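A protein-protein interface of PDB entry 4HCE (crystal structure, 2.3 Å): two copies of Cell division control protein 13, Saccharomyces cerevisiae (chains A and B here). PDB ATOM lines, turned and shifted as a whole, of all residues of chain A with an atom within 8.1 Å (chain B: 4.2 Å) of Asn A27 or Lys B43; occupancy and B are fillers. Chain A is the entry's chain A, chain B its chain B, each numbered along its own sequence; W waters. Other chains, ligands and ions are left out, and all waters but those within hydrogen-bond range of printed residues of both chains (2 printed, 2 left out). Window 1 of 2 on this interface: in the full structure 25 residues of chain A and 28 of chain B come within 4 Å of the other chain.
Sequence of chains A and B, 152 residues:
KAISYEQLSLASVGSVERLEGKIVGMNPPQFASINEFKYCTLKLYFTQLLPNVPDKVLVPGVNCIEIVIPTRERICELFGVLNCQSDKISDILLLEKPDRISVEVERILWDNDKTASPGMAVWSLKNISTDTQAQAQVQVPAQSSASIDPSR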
ATOM      1  N   ILE A  23      26.288  28.034 -31.204  1.00  0.00           N
ATOM      2  CA  ILE A  23      26.210  28.015 -29.742  1.00  0.00           C
ATOM      3  C   ILE A  23      24.735  28.225 -29.400  1.00  0.00           C
ATOM      4  O   ILE A  23      24.140  29.255 -29.763  1.00  0.00           O
ATOM      5  CB  ILE A  23      27.084  29.103 -29.046  1.00  0.00           C
ATOM      6  CG1 ILE A  23      28.570  29.015 -29.473  1.00  0.00           C
ATOM      7  CG2 ILE A  23      26.932  29.031 -27.522  1.00  0.00           C
ATOM      8  CD1 ILE A  23      29.219  27.649 -29.307  1.00  0.00           C
ATOM      9  N   GLY A  25      23.451  27.503 -26.104  1.00  0.00           N
ATOM     10  CA  GLY A  25      23.303  27.851 -24.697  1.00  0.00           C
ATOM     11  C   GLY A  25      24.630  28.000 -23.975  1.00  0.00           C
ATOM     12  O   GLY A  25      25.700  27.732 -24.538  1.00  0.00           O
ATOM     13  N   MET A  26      24.550  28.437 -22.722  1.00  0.00           N
ATOM     14  CA  MET A  26      25.706  28.556 -21.862  1.00  0.00           C
ATOM     15  C   MET A  26      25.374  28.123 -20.443  1.00  0.00           C
ATOM     16  O   MET A  26      24.244  28.272 -19.989  1.00  0.00           O
ATOM     17  CB  MET A  26      26.309  29.975 -21.898  1.00  0.00           C
ATOM     18  CG  MET A  26      25.572  31.068 -21.128  1.00  0.00           C
ATOM     19  SD  MET A  26      26.273  32.724 -21.459  1.00  0.00           S
ATOM     20  CE  MET A  26      25.530  33.042 -23.042  1.00  0.00           C
ATOM     21  N   ASN A  27      26.386  27.603 -19.757  1.00  0.00           N
ATOM     22  CA  ASN A  27      26.289  27.235 -18.363  1.00  0.00           C
ATOM     23  C   ASN A  27      27.459  27.805 -17.525  1.00  0.00           C
ATOM     24  O   ASN A  27      28.624  27.616 -17.882  1.00  0.00           O
ATOM     25  CB  ASN A  27      26.279  25.718 -18.261  1.00  0.00           C
ATOM     26  CG  ASN A  27      25.591  25.239 -17.019  1.00  0.00           C
ATOM     27  OD1 ASN A  27      24.351  25.141 -16.973  1.00  0.00           O
ATOM     28  ND2 ASN A  27      26.383  24.954 -15.982  1.00  0.00           N
ATOM     29  N   PRO A  28      27.157  28.527 -16.426  1.00  0.00           N
ATOM     30  CA  PRO A  28      25.816  28.917 -15.947  1.00  0.00           C
ATOM     31  C   PRO A  28      25.122  29.847 -16.947  1.00  0.00           C
ATOM     32  O   PRO A  28      25.804  30.576 -17.692  1.00  0.00           O
ATOM     33  CB  PRO A  28      26.090  29.681 -14.635  1.00  0.00           C
ATOM     34  CG  PRO A  28      27.538  29.562 -14.364  1.00  0.00           C
ATOM     35  CD  PRO A  28      28.236  29.109 -15.610  1.00  0.00           C
ATOM     36  N   PRO A  29      23.779  29.821 -16.970  1.00  0.00           N
ATOM     37  CA  PRO A  29      23.048  30.574 -17.970  1.00  0.00           C
ATOM     38  C   PRO A  29      22.840  32.016 -17.531  1.00  0.00           C
ATOM     39  O   PRO A  29      22.468  32.875 -18.359  1.00  0.00           O
ATOM     40  CB  PRO A  29      21.714  29.832 -18.056  1.00  0.00           C
ATOM     41  CG  PRO A  29      21.517  29.238 -16.698  1.00  0.00           C
ATOM     42  CD  PRO A  29      22.892  28.970 -16.145  1.00  0.00           C
ATOM     43  N   GLN A  30      23.075  32.271 -16.242  1.00  0.00           N
ATOM     44  CA  GLN A  30      23.048  33.626 -15.716  1.00  0.00           C
ATOM     45  C   GLN A  30      24.281  33.883 -14.854  1.00  0.00           C
ATOM     46  O   GLN A  30      24.697  33.008 -14.088  1.00  0.00           O
ATOM     47  CB  GLN A  30      21.763  33.867 -14.935  1.00  0.00           C
ATOM     48  CG  GLN A  30      20.944  35.047 -15.438  1.00  0.00           C
ATOM     49  CD  GLN A  30      19.688  35.283 -14.615  1.00  0.00           C
ATOM     50  OE1 GLN A  30      18.665  34.600 -14.786  1.00  0.00           O
ATOM     51  NE2 GLN A  30      19.757  36.256 -13.712  1.00  0.00           N
ATOM     52  N   PHE A  31      24.889  35.062 -15.026  1.00  0.00           N
ATOM     53  CA  PHE A  31      26.050  35.507 -14.231  1.00  0.00           C
ATOM     54  C   PHE A  31      26.344  36.996 -14.404  1.00  0.00           C
ATOM     55  O   PHE A  31      26.056  37.579 -15.457  1.00  0.00           O
ATOM     56  CB  PHE A  31      27.319  34.674 -14.514  1.00  0.00           C
ATOM     57  CG  PHE A  31      27.703  34.609 -15.968  1.00  0.00           C
ATOM     58  CD1 PHE A  31      28.447  35.641 -16.561  1.00  0.00           C
ATOM     59  CD2 PHE A  31      27.342  33.517 -16.740  1.00  0.00           C
ATOM     60  CE1 PHE A  31      28.801  35.584 -17.901  1.00  0.00           C
ATOM     61  CE2 PHE A  31      27.705  33.447 -18.080  1.00  0.00           C
ATOM     62  CZ  PHE A  31      28.422  34.482 -18.663  1.00  0.00           C
ATOM     63  N   PHE A  37      33.628  32.977 -11.813  1.00  0.00           N
ATOM     64  CA  PHE A  37      34.363  31.907 -12.451  1.00  0.00           C
ATOM     65  C   PHE A  37      35.678  31.555 -11.747  1.00  0.00           C
ATOM     66  O   PHE A  37      36.588  30.980 -12.358  1.00  0.00           O
ATOM     67  CB  PHE A  37      34.518  32.201 -13.949  1.00  0.00           C
ATOM     68  CG  PHE A  37      33.197  32.354 -14.652  1.00  0.00           C
ATOM     69  CD1 PHE A  37      32.728  33.608 -15.024  1.00  0.00           C
ATOM     70  CD2 PHE A  37      32.387  31.240 -14.887  1.00  0.00           C
ATOM     71  CE1 PHE A  37      31.489  33.745 -15.639  1.00  0.00           C
ATOM     72  CE2 PHE A  37      31.149  31.379 -15.491  1.00  0.00           C
ATOM     73  CZ  PHE A  37      30.704  32.634 -15.872  1.00  0.00           C
ATOM     74  N   CYS A  40      33.802  27.965 -10.410  1.00  0.00           N
ATOM     75  CA  CYS A  40      32.899  27.601 -11.478  1.00  0.00           C
ATOM     76  C   CYS A  40      33.507  27.852 -12.853  1.00  0.00           C
ATOM     77  O   CYS A  40      34.294  28.770 -13.029  1.00  0.00           O
ATOM     78  CB  CYS A  40      31.609  28.398 -11.375  1.00  0.00           C
ATOM     79  SG  CYS A  40      30.238  27.490 -12.092  1.00  0.00           S
ATOM     80  N   THR A  41      33.098  27.041 -13.820  1.00  0.00           N
ATOM     81  CA  THR A  41      33.645  27.085 -15.161  1.00  0.00           C
ATOM     82  C   THR A  41      32.576  27.452 -16.172  1.00  0.00           C
ATOM     83  O   THR A  41      31.461  26.933 -16.128  1.00  0.00           O
ATOM     84  CB  THR A  41      34.264  25.720 -15.521  1.00  0.00           C
ATOM     85  OG1 THR A  41      35.441  25.522 -14.722  1.00  0.00           O
ATOM     86  CG2 THR A  41      34.630  25.625 -17.001  1.00  0.00           C
ATOM     87  N   LEU A  42      32.928  28.335 -17.100  1.00  0.00           N
ATOM     88  CA  LEU A  42      31.990  28.708 -18.142  1.00  0.00           C
ATOM     89  C   LEU A  42      31.994  27.629 -19.227  1.00  0.00           C
ATOM     90  O   LEU A  42      33.060  27.201 -19.688  1.00  0.00           O
ATOM     91  CB  LEU A  42      32.336  30.084 -18.710  1.00  0.00           C
ATOM     92  CG  LEU A  42      31.458  30.507 -19.895  1.00  0.00           C
ATOM     93  CD1 LEU A  42      30.050  30.803 -19.404  1.00  0.00           C
ATOM     94  CD2 LEU A  42      32.078  31.717 -20.571  1.00  0.00           C
ATOM     95  N   LYS A  43      30.799  27.167 -19.590  1.00  0.00           N
ATOM     96  CA  LYS A  43      30.606  26.134 -20.604  1.00  0.00           C
ATOM     97  C   LYS A  43      29.649  26.647 -21.659  1.00  0.00           C
ATOM     98  O   LYS A  43      28.663  27.319 -21.342  1.00  0.00           O
ATOM     99  CB  LYS A  43      30.016  24.868 -19.976  1.00  0.00           C
ATOM    100  CG  LYS A  43      30.877  24.272 -18.876  1.00  0.00           C
ATOM    101  CD  LYS A  43      30.036  23.569 -17.825  1.00  0.00           C
ATOM    102  CE  LYS A  43      30.906  23.142 -16.652  1.00  0.00           C
ATOM    103  NZ  LYS A  43      31.125  24.221 -15.634  1.00  0.00           N
ATOM    104  N   LEU A  44      29.945  26.329 -22.914  1.00  0.00           N
ATOM    105  CA  LEU A  44      29.067  26.672 -24.036  1.00  0.00           C
ATOM    106  C   LEU A  44      28.596  25.371 -24.683  1.00  0.00           C
ATOM    107  O   LEU A  44      29.284  24.342 -24.586  1.00  0.00           O
ATOM    108  CB  LEU A  44      29.805  27.574 -25.045  1.00  0.00           C
ATOM    109  CG  LEU A  44      30.592  28.794 -24.510  1.00  0.00           C
ATOM    110  CD1 LEU A  44      31.255  29.571 -25.646  1.00  0.00           C
ATOM    111  CD2 LEU A  44      29.738  29.732 -23.658  1.00  0.00           C
ATOM    112  N   TYR A  45      27.427  25.400 -25.321  1.00  0.00           N
ATOM    113  CA  TYR A  45      26.855  24.196 -25.915  1.00  0.00           C
ATOM    114  C   TYR A  45      26.724  24.376 -27.406  1.00  0.00           C
ATOM    115  O   TYR A  45      26.041  25.283 -27.879  1.00  0.00           O
ATOM    116  CB  TYR A  45      25.509  23.833 -25.270  1.00  0.00           C
ATOM    117  CG  TYR A  45      25.645  23.517 -23.800  1.00  0.00           C
ATOM    118  CD1 TYR A  45      26.255  22.339 -23.378  1.00  0.00           C
ATOM    119  CD2 TYR A  45      25.208  24.428 -22.823  1.00  0.00           C
ATOM    120  CE1 TYR A  45      26.424  22.069 -22.029  1.00  0.00           C
ATOM    121  CE2 TYR A  45      25.352  24.157 -21.469  1.00  0.00           C
ATOM    122  CZ  TYR A  45      25.969  22.983 -21.082  1.00  0.00           C
ATOM    123  OH  TYR A  45      26.116  22.691 -19.742  1.00  0.00           O
ATOM    124  N   GLU A  66      29.581  20.041 -25.170  1.00  0.00           N
ATOM    125  CA  GLU A  66      29.902  21.043 -24.193  1.00  0.00           C
ATOM    126  C   GLU A  66      31.326  21.538 -24.451  1.00  0.00           C
ATOM    127  O   GLU A  66      32.278  20.744 -24.582  1.00  0.00           O
ATOM    128  CB  GLU A  66      29.762  20.432 -22.810  1.00  0.00           C
ATOM    129  CG  GLU A  66      30.441  21.183 -21.699  1.00  0.00           C
ATOM    130  CD  GLU A  66      30.607  20.305 -20.472  1.00  0.00           C
ATOM    131  OE1 GLU A  66      29.637  20.237 -19.684  1.00  0.00           O
ATOM    132  OE2 GLU A  66      31.702  19.692 -20.317  1.00  0.00           O
ATOM    133  N   ILE A  67      31.466  22.855 -24.547  1.00  0.00           N
ATOM    134  CA  ILE A  67      32.778  23.489 -24.733  1.00  0.00           C
ATOM    135  C   ILE A  67      33.086  24.289 -23.453  1.00  0.00           C
ATOM    136  O   ILE A  67      32.287  25.144 -23.056  1.00  0.00           O
ATOM    137  CB  ILE A  67      32.779  24.404 -25.982  1.00  0.00           C
ATOM    138  CG1 ILE A  67      32.270  23.648 -27.219  1.00  0.00           C
ATOM    139  CG2 ILE A  67      34.164  24.965 -26.266  1.00  0.00           C
ATOM    140  CD1 ILE A  67      32.128  24.519 -28.455  1.00  0.00           C
ATOM    141  N   VAL A  68      34.194  23.964 -22.777  1.00  0.00           N
ATOM    142  CA  VAL A  68      34.598  24.704 -21.574  1.00  0.00           C
ATOM    143  C   VAL A  68      35.577  25.833 -21.923  1.00  0.00           C
ATOM    144  O   VAL A  68      36.397  25.701 -22.847  1.00  0.00           O
ATOM    145  CB  VAL A  68      35.190  23.806 -20.443  1.00  0.00           C
ATOM    146  CG1 VAL A  68      34.333  22.557 -20.186  1.00  0.00           C
ATOM    147  CG2 VAL A  68      36.635  23.435 -20.726  1.00  0.00           C
ATOM    148  N   ILE A  69      35.436  26.958 -21.236  1.00  0.00           N
ATOM    149  CA  ILE A  69      36.428  28.023 -21.290  1.00  0.00           C
ATOM    150  C   ILE A  69      37.116  27.909 -19.930  1.00  0.00           C
ATOM    151  O   ILE A  69      36.628  28.455 -18.949  1.00  0.00           O
ATOM    152  CB  ILE A  69      35.822  29.441 -21.470  1.00  0.00           C
ATOM    153  CG1 ILE A  69      34.641  29.478 -22.479  1.00  0.00           C
ATOM    154  CG2 ILE A  69      36.915  30.463 -21.763  1.00  0.00           C
ATOM    155  CD1 ILE A  69      34.964  29.212 -23.928  1.00  0.00           C
ATOM    156  N   LEU A  95      23.292  34.001 -29.669  1.00  0.00           N
ATOM    157  CA  LEU A  95      22.452  32.850 -29.329  1.00  0.00           C
ATOM    158  C   LEU A  95      20.958  33.050 -29.640  1.00  0.00           C
ATOM    159  O   LEU A  95      20.137  32.147 -29.494  1.00  0.00           O
ATOM    160  CB  LEU A  95      22.521  32.594 -27.820  1.00  0.00           C
ATOM    161  CG  LEU A  95      23.851  32.110 -27.231  1.00  0.00           C
ATOM    162  CD1 LEU A  95      25.029  32.974 -27.652  1.00  0.00           C
ATOM    163  CD2 LEU A  95      23.755  32.060 -25.717  1.00  0.00           C
ATOM    164  N   MET A 120      39.720  15.461 -16.310  1.00  0.00           N
ATOM    165  CA  MET A 120      38.690  15.057 -17.233  1.00  0.00           C
ATOM    166  C   MET A 120      39.076  15.460 -18.640  1.00  0.00           C
ATOM    167  O   MET A 120      39.607  16.564 -18.848  1.00  0.00           O
ATOM    168  CB  MET A 120      37.386  15.744 -16.876  1.00  0.00           C
ATOM    169  CG  MET A 120      36.717  15.194 -15.635  1.00  0.00           C
ATOM    170  SD  MET A 120      35.162  16.051 -15.342  1.00  0.00           S
ATOM    171  CE  MET A 120      35.831  17.646 -14.889  1.00  0.00           C
ATOM    172  N   MET B  26      34.224  15.564  -7.795  1.00  0.00           N
ATOM    173  CA  MET B  26      33.175  16.551  -7.804  1.00  0.00           C
ATOM    174  C   MET B  26      33.599  17.798  -8.559  1.00  0.00           C
ATOM    175  O   MET B  26      34.788  18.127  -8.653  1.00  0.00           O
ATOM    176  CB  MET B  26      32.668  16.874  -6.378  1.00  0.00           C
ATOM    177  CG  MET B  26      33.619  17.628  -5.470  1.00  0.00           C
ATOM    178  SD  MET B  26      33.051  17.775  -3.746  1.00  0.00           S
ATOM    179  CE  MET B  26      34.628  17.903  -2.937  1.00  0.00           C
ATOM    180  N   ASN B  27      32.596  18.464  -9.109  1.00  0.00           N
ATOM    181  CA  ASN B  27      32.774  19.705  -9.816  1.00  0.00           C
ATOM    182  C   ASN B  27      31.751  20.743  -9.330  1.00  0.00           C
ATOM    183  O   ASN B  27      30.537  20.460  -9.308  1.00  0.00           O
ATOM    184  CB  ASN B  27      32.576  19.468 -11.294  1.00  0.00           C
ATOM    185  CG  ASN B  27      33.301  20.480 -12.131  1.00  0.00           C
ATOM    186  OD1 ASN B  27      34.516  20.378 -12.316  1.00  0.00           O
ATOM    187  ND2 ASN B  27      32.573  21.471 -12.635  1.00  0.00           N
ATOM    188  N   THR B  41      26.599  24.961 -10.385  1.00  0.00           N
ATOM    189  CA  THR B  41      25.967  23.705  -9.979  1.00  0.00           C
ATOM    190  C   THR B  41      26.991  22.682  -9.445  1.00  0.00           C
ATOM    191  O   THR B  41      28.097  22.565  -9.962  1.00  0.00           O
ATOM    192  CB  THR B  41      25.128  23.135 -11.141  1.00  0.00           C
ATOM    193  OG1 THR B  41      24.071  24.062 -11.423  1.00  0.00           O
ATOM    194  CG2 THR B  41      24.520  21.790 -10.796  1.00  0.00           C
ATOM    195  N   LEU B  42      26.619  21.985  -8.380  1.00  0.00           N
ATOM    196  CA  LEU B  42      27.444  20.929  -7.844  1.00  0.00           C
ATOM    197  C   LEU B  42      27.173  19.652  -8.629  1.00  0.00           C
ATOM    198  O   LEU B  42      26.017  19.227  -8.775  1.00  0.00           O
ATOM    199  CB  LEU B  42      27.187  20.740  -6.347  1.00  0.00           C
ATOM    200  CG  LEU B  42      27.927  19.602  -5.633  1.00  0.00           C
ATOM    201  CD1 LEU B  42      29.434  19.862  -5.584  1.00  0.00           C
ATOM    202  CD2 LEU B  42      27.352  19.447  -4.232  1.00  0.00           C
ATOM    203  N   LYS B  43      28.248  19.073  -9.150  1.00  0.00           N
ATOM    204  CA  LYS B  43      28.206  17.836  -9.921  1.00  0.00           C
ATOM    205  C   LYS B  43      29.088  16.785  -9.262  1.00  0.00           C
ATOM    206  O   LYS B  43      30.185  17.103  -8.753  1.00  0.00           O
ATOM    207  CB  LYS B  43      28.689  18.075 -11.356  1.00  0.00           C
ATOM    208  CG  LYS B  43      27.782  19.005 -12.154  1.00  0.00           C
ATOM    209  CD  LYS B  43      28.531  19.657 -13.303  1.00  0.00           C
ATOM    210  CE  LYS B  43      28.144  21.122 -13.455  1.00  0.00           C
ATOM    211  NZ  LYS B  43      27.265  21.416 -14.637  1.00  0.00           N
ATOM    212  N   LEU B  44      28.598  15.544  -9.244  1.00  0.00           N
ATOM    213  CA  LEU B  44      29.405  14.414  -8.752  1.00  0.00           C
ATOM    214  C   LEU B  44      29.711  13.446  -9.876  1.00  0.00           C
ATOM    215  O   LEU B  44      28.899  13.281 -10.787  1.00  0.00           O
ATOM    216  CB  LEU B  44      28.699  13.688  -7.614  1.00  0.00           C
ATOM    217  CG  LEU B  44      28.217  14.559  -6.448  1.00  0.00           C
ATOM    218  CD1 LEU B  44      27.494  13.649  -5.463  1.00  0.00           C
ATOM    219  CD2 LEU B  44      29.345  15.306  -5.758  1.00  0.00           C
ATOM    220  N   GLU B  66      27.982  11.892 -14.767  1.00  0.00           N
ATOM    221  CA  GLU B  66      27.806  13.143 -14.057  1.00  0.00           C
ATOM    222  C   GLU B  66      26.443  13.139 -13.322  1.00  0.00           C
ATOM    223  O   GLU B  66      25.415  12.821 -13.891  1.00  0.00           O
ATOM    224  CB  GLU B  66      27.902  14.307 -15.058  1.00  0.00           C
ATOM    225  CG  GLU B  66      27.380  15.624 -14.507  1.00  0.00           C
ATOM    226  CD  GLU B  66      27.012  16.622 -15.611  1.00  0.00           C
ATOM    227  OE1 GLU B  66      25.788  16.785 -15.959  1.00  0.00           O
ATOM    228  OE2 GLU B  66      27.965  17.227 -16.135  1.00  0.00           O
ATOM    229  N   ILE B  67      26.443  13.504 -12.054  1.00  0.00           N
ATOM    230  CA  ILE B  67      25.209  13.595 -11.276  1.00  0.00           C
ATOM    231  C   ILE B  67      25.119  15.016 -10.719  1.00  0.00           C
ATOM    232  O   ILE B  67      26.016  15.466  -9.994  1.00  0.00           O
ATOM    233  CB  ILE B  67      25.203  12.603 -10.104  1.00  0.00           C
ATOM    234  CG1 ILE B  67      25.465  11.161 -10.584  1.00  0.00           C
ATOM    235  CG2 ILE B  67      23.887  12.692  -9.338  1.00  0.00           C
ATOM    236  CD1 ILE B  67      25.781  10.191  -9.447  1.00  0.00           C
ATOM    237  N   VAL B  68      24.046  15.719 -11.068  1.00  0.00           N
ATOM    238  CA  VAL B  68      23.844  17.062 -10.590  1.00  0.00           C
ATOM    239  C   VAL B  68      23.009  17.035  -9.326  1.00  0.00           C
ATOM    240  O   VAL B  68      22.043  16.247  -9.219  1.00  0.00           O
ATOM    241  CB  VAL B  68      23.252  18.033 -11.667  1.00  0.00           C
ATOM    242  CG1 VAL B  68      23.978  17.897 -12.998  1.00  0.00           C
ATOM    243  CG2 VAL B  68      21.780  17.782 -11.901  1.00  0.00           C
ATOM    244  N   TRP B 110      16.235  19.632 -16.773  1.00  0.00           N
ATOM    245  CA  TRP B 110      16.765  20.608 -15.875  1.00  0.00           C
ATOM    246  C   TRP B 110      16.720  21.911 -16.596  1.00  0.00           C
ATOM    247  O   TRP B 110      17.540  22.190 -17.474  1.00  0.00           O
ATOM    248  CB  TRP B 110      18.173  20.207 -15.490  1.00  0.00           C
ATOM    249  CG  TRP B 110      18.867  21.171 -14.570  1.00  0.00           C
ATOM    250  CD1 TRP B 110      18.324  21.878 -13.497  1.00  0.00           C
ATOM    251  CD2 TRP B 110      20.284  21.556 -14.606  1.00  0.00           C
ATOM    252  NE1 TRP B 110      19.274  22.659 -12.896  1.00  0.00           N
ATOM    253  CE2 TRP B 110      20.474  22.513 -13.510  1.00  0.00           C
ATOM    254  CE3 TRP B 110      21.374  21.220 -15.412  1.00  0.00           C
ATOM    255  CZ2 TRP B 110      21.714  23.090 -13.246  1.00  0.00           C
ATOM    256  CZ3 TRP B 110      22.621  21.804 -15.132  1.00  0.00           C
ATOM    257  CH2 TRP B 110      22.786  22.716 -14.074  1.00  0.00           C
ATOM    258  N   ASN B 112      16.950  25.717 -16.398  1.00  0.00           N
ATOM    259  CA  ASN B 112      17.723  26.506 -15.441  1.00  0.00           C
ATOM    260  C   ASN B 112      17.029  27.693 -14.796  1.00  0.00           C
ATOM    261  O   ASN B 112      16.502  27.579 -13.686  1.00  0.00           O
ATOM    262  CB  ASN B 112      19.061  26.956 -16.049  1.00  0.00           C
ATOM    263  CG  ASN B 112      20.156  25.915 -15.905  1.00  0.00           C
ATOM    264  OD1 ASN B 112      21.140  26.133 -15.192  1.00  0.00           O
ATOM    265  ND2 ASN B 112      19.995  24.777 -16.581  1.00  0.00           N
ATOM    266  N   MET B 120      18.155  20.997 -20.310  1.00  0.00           N
ATOM    267  CA  MET B 120      18.878  19.807 -20.757  1.00  0.00           C
ATOM    268  C   MET B 120      18.533  18.601 -19.913  1.00  0.00           C
ATOM    269  O   MET B 120      17.995  18.746 -18.825  1.00  0.00           O
ATOM    270  CB  MET B 120      20.395  20.041 -20.851  1.00  0.00           C
ATOM    271  CG  MET B 120      21.030  20.764 -19.689  1.00  0.00           C
ATOM    272  SD  MET B 120      22.584  21.508 -20.235  1.00  0.00           S
ATOM    273  CE  MET B 120      22.992  22.462 -18.779  1.00  0.00           C
HETATM  274  O   HOH W   1      24.400  26.077 -13.357  1.00  0.00           O
HETATM  275  O   HOH W   2      27.180  24.770 -13.333  1.00  0.00           O
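The side-chain hydroxyl (OH) of Tyr A45 sits close to the side-chain sulfur (SD) of Met B120.
O of Gly A25 lies within hydrogen-bond range of N of Tyr A45, at 3.0 Å.
The backbone NH of Asn A27 is in hydrogen-bond range of the backbone carbonyl oxygen of Lys A43 (2.8 Å).
The backbone carbonyl oxygen of Asn B27 lies within hydrogen-bond range of the backbone NH of Lys B43 (2.7 Å).
N of Trp B110 is in hydrogen-bond range of O of Met B120.
Among the printed residues, pairs that only touch across the chains: Pro A29 with Asn B112 (3.4 Å), Asn A27 with Met B120 (3.5 Å), Asn A27 with Asn B112 (3.8 Å), Asn A27 with Lys B43 (3.9 Å) and Met A120 with Asn B27 (3.98 Å).
Asn A27 touches three residues of chain B.
Of the printed residues of chain B, Pro A29 touches Asn B112.
Of the printed residues of chain A, Asn B27 touches Met A120.
Of the printed residues of chain B, Met A120 touches Asn B27 (3.98 Å).
Printed residues of chain B within 4 Å of Tyr A45: Met B120 (3.3 Å).
Of the printed residues of chain A, Met B120 touches Asn A27 (3.5 Å) and Tyr A45 (3.3 Å).
The nearest residue of chain A that does not touch Lys B43 is Lys A43 (4.5 Å).
Hydrophobic or aromatic side chains of chain A within 4 Å of the printed part of chain B: Pro A29, Tyr A45 and Met A120.
Of the 12 printed residues of chain B, 4 touch a printed residue of chain A.
Hydrophobic or aromatic side chains of chain B that line the printed part of chain A: Met B120.
Among the printed residues, no Asp or Glu carboxylate lies within 4 Å of a Lys or Arg side-chain nitrogen of the other chain.
Asn A27 touches Lys B43, but with the chains exchanged Lys A43 does not touch Asn B27 (4.3 Å).
Asn A27 touches Met B120, and with the chains exchanged Met A120 touches Asn B27.
Positions printed for both chains: 26, 27, 41, 42, 43, 44, 66, 67, 68 and 120.
Of the 6 pairs that touch across the chains among the printed residues, 2 have their exchanged pair printed and touching as well.
Water W2 bridges ND2 of Asn A27 (2.8 Å) and N of Thr B41 (3.0 Å).
Water W1 lies within hydrogen-bond range of OG1 of Thr B41 (2.8 Å) and ND2 of Asn A27 (3.5 Å).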
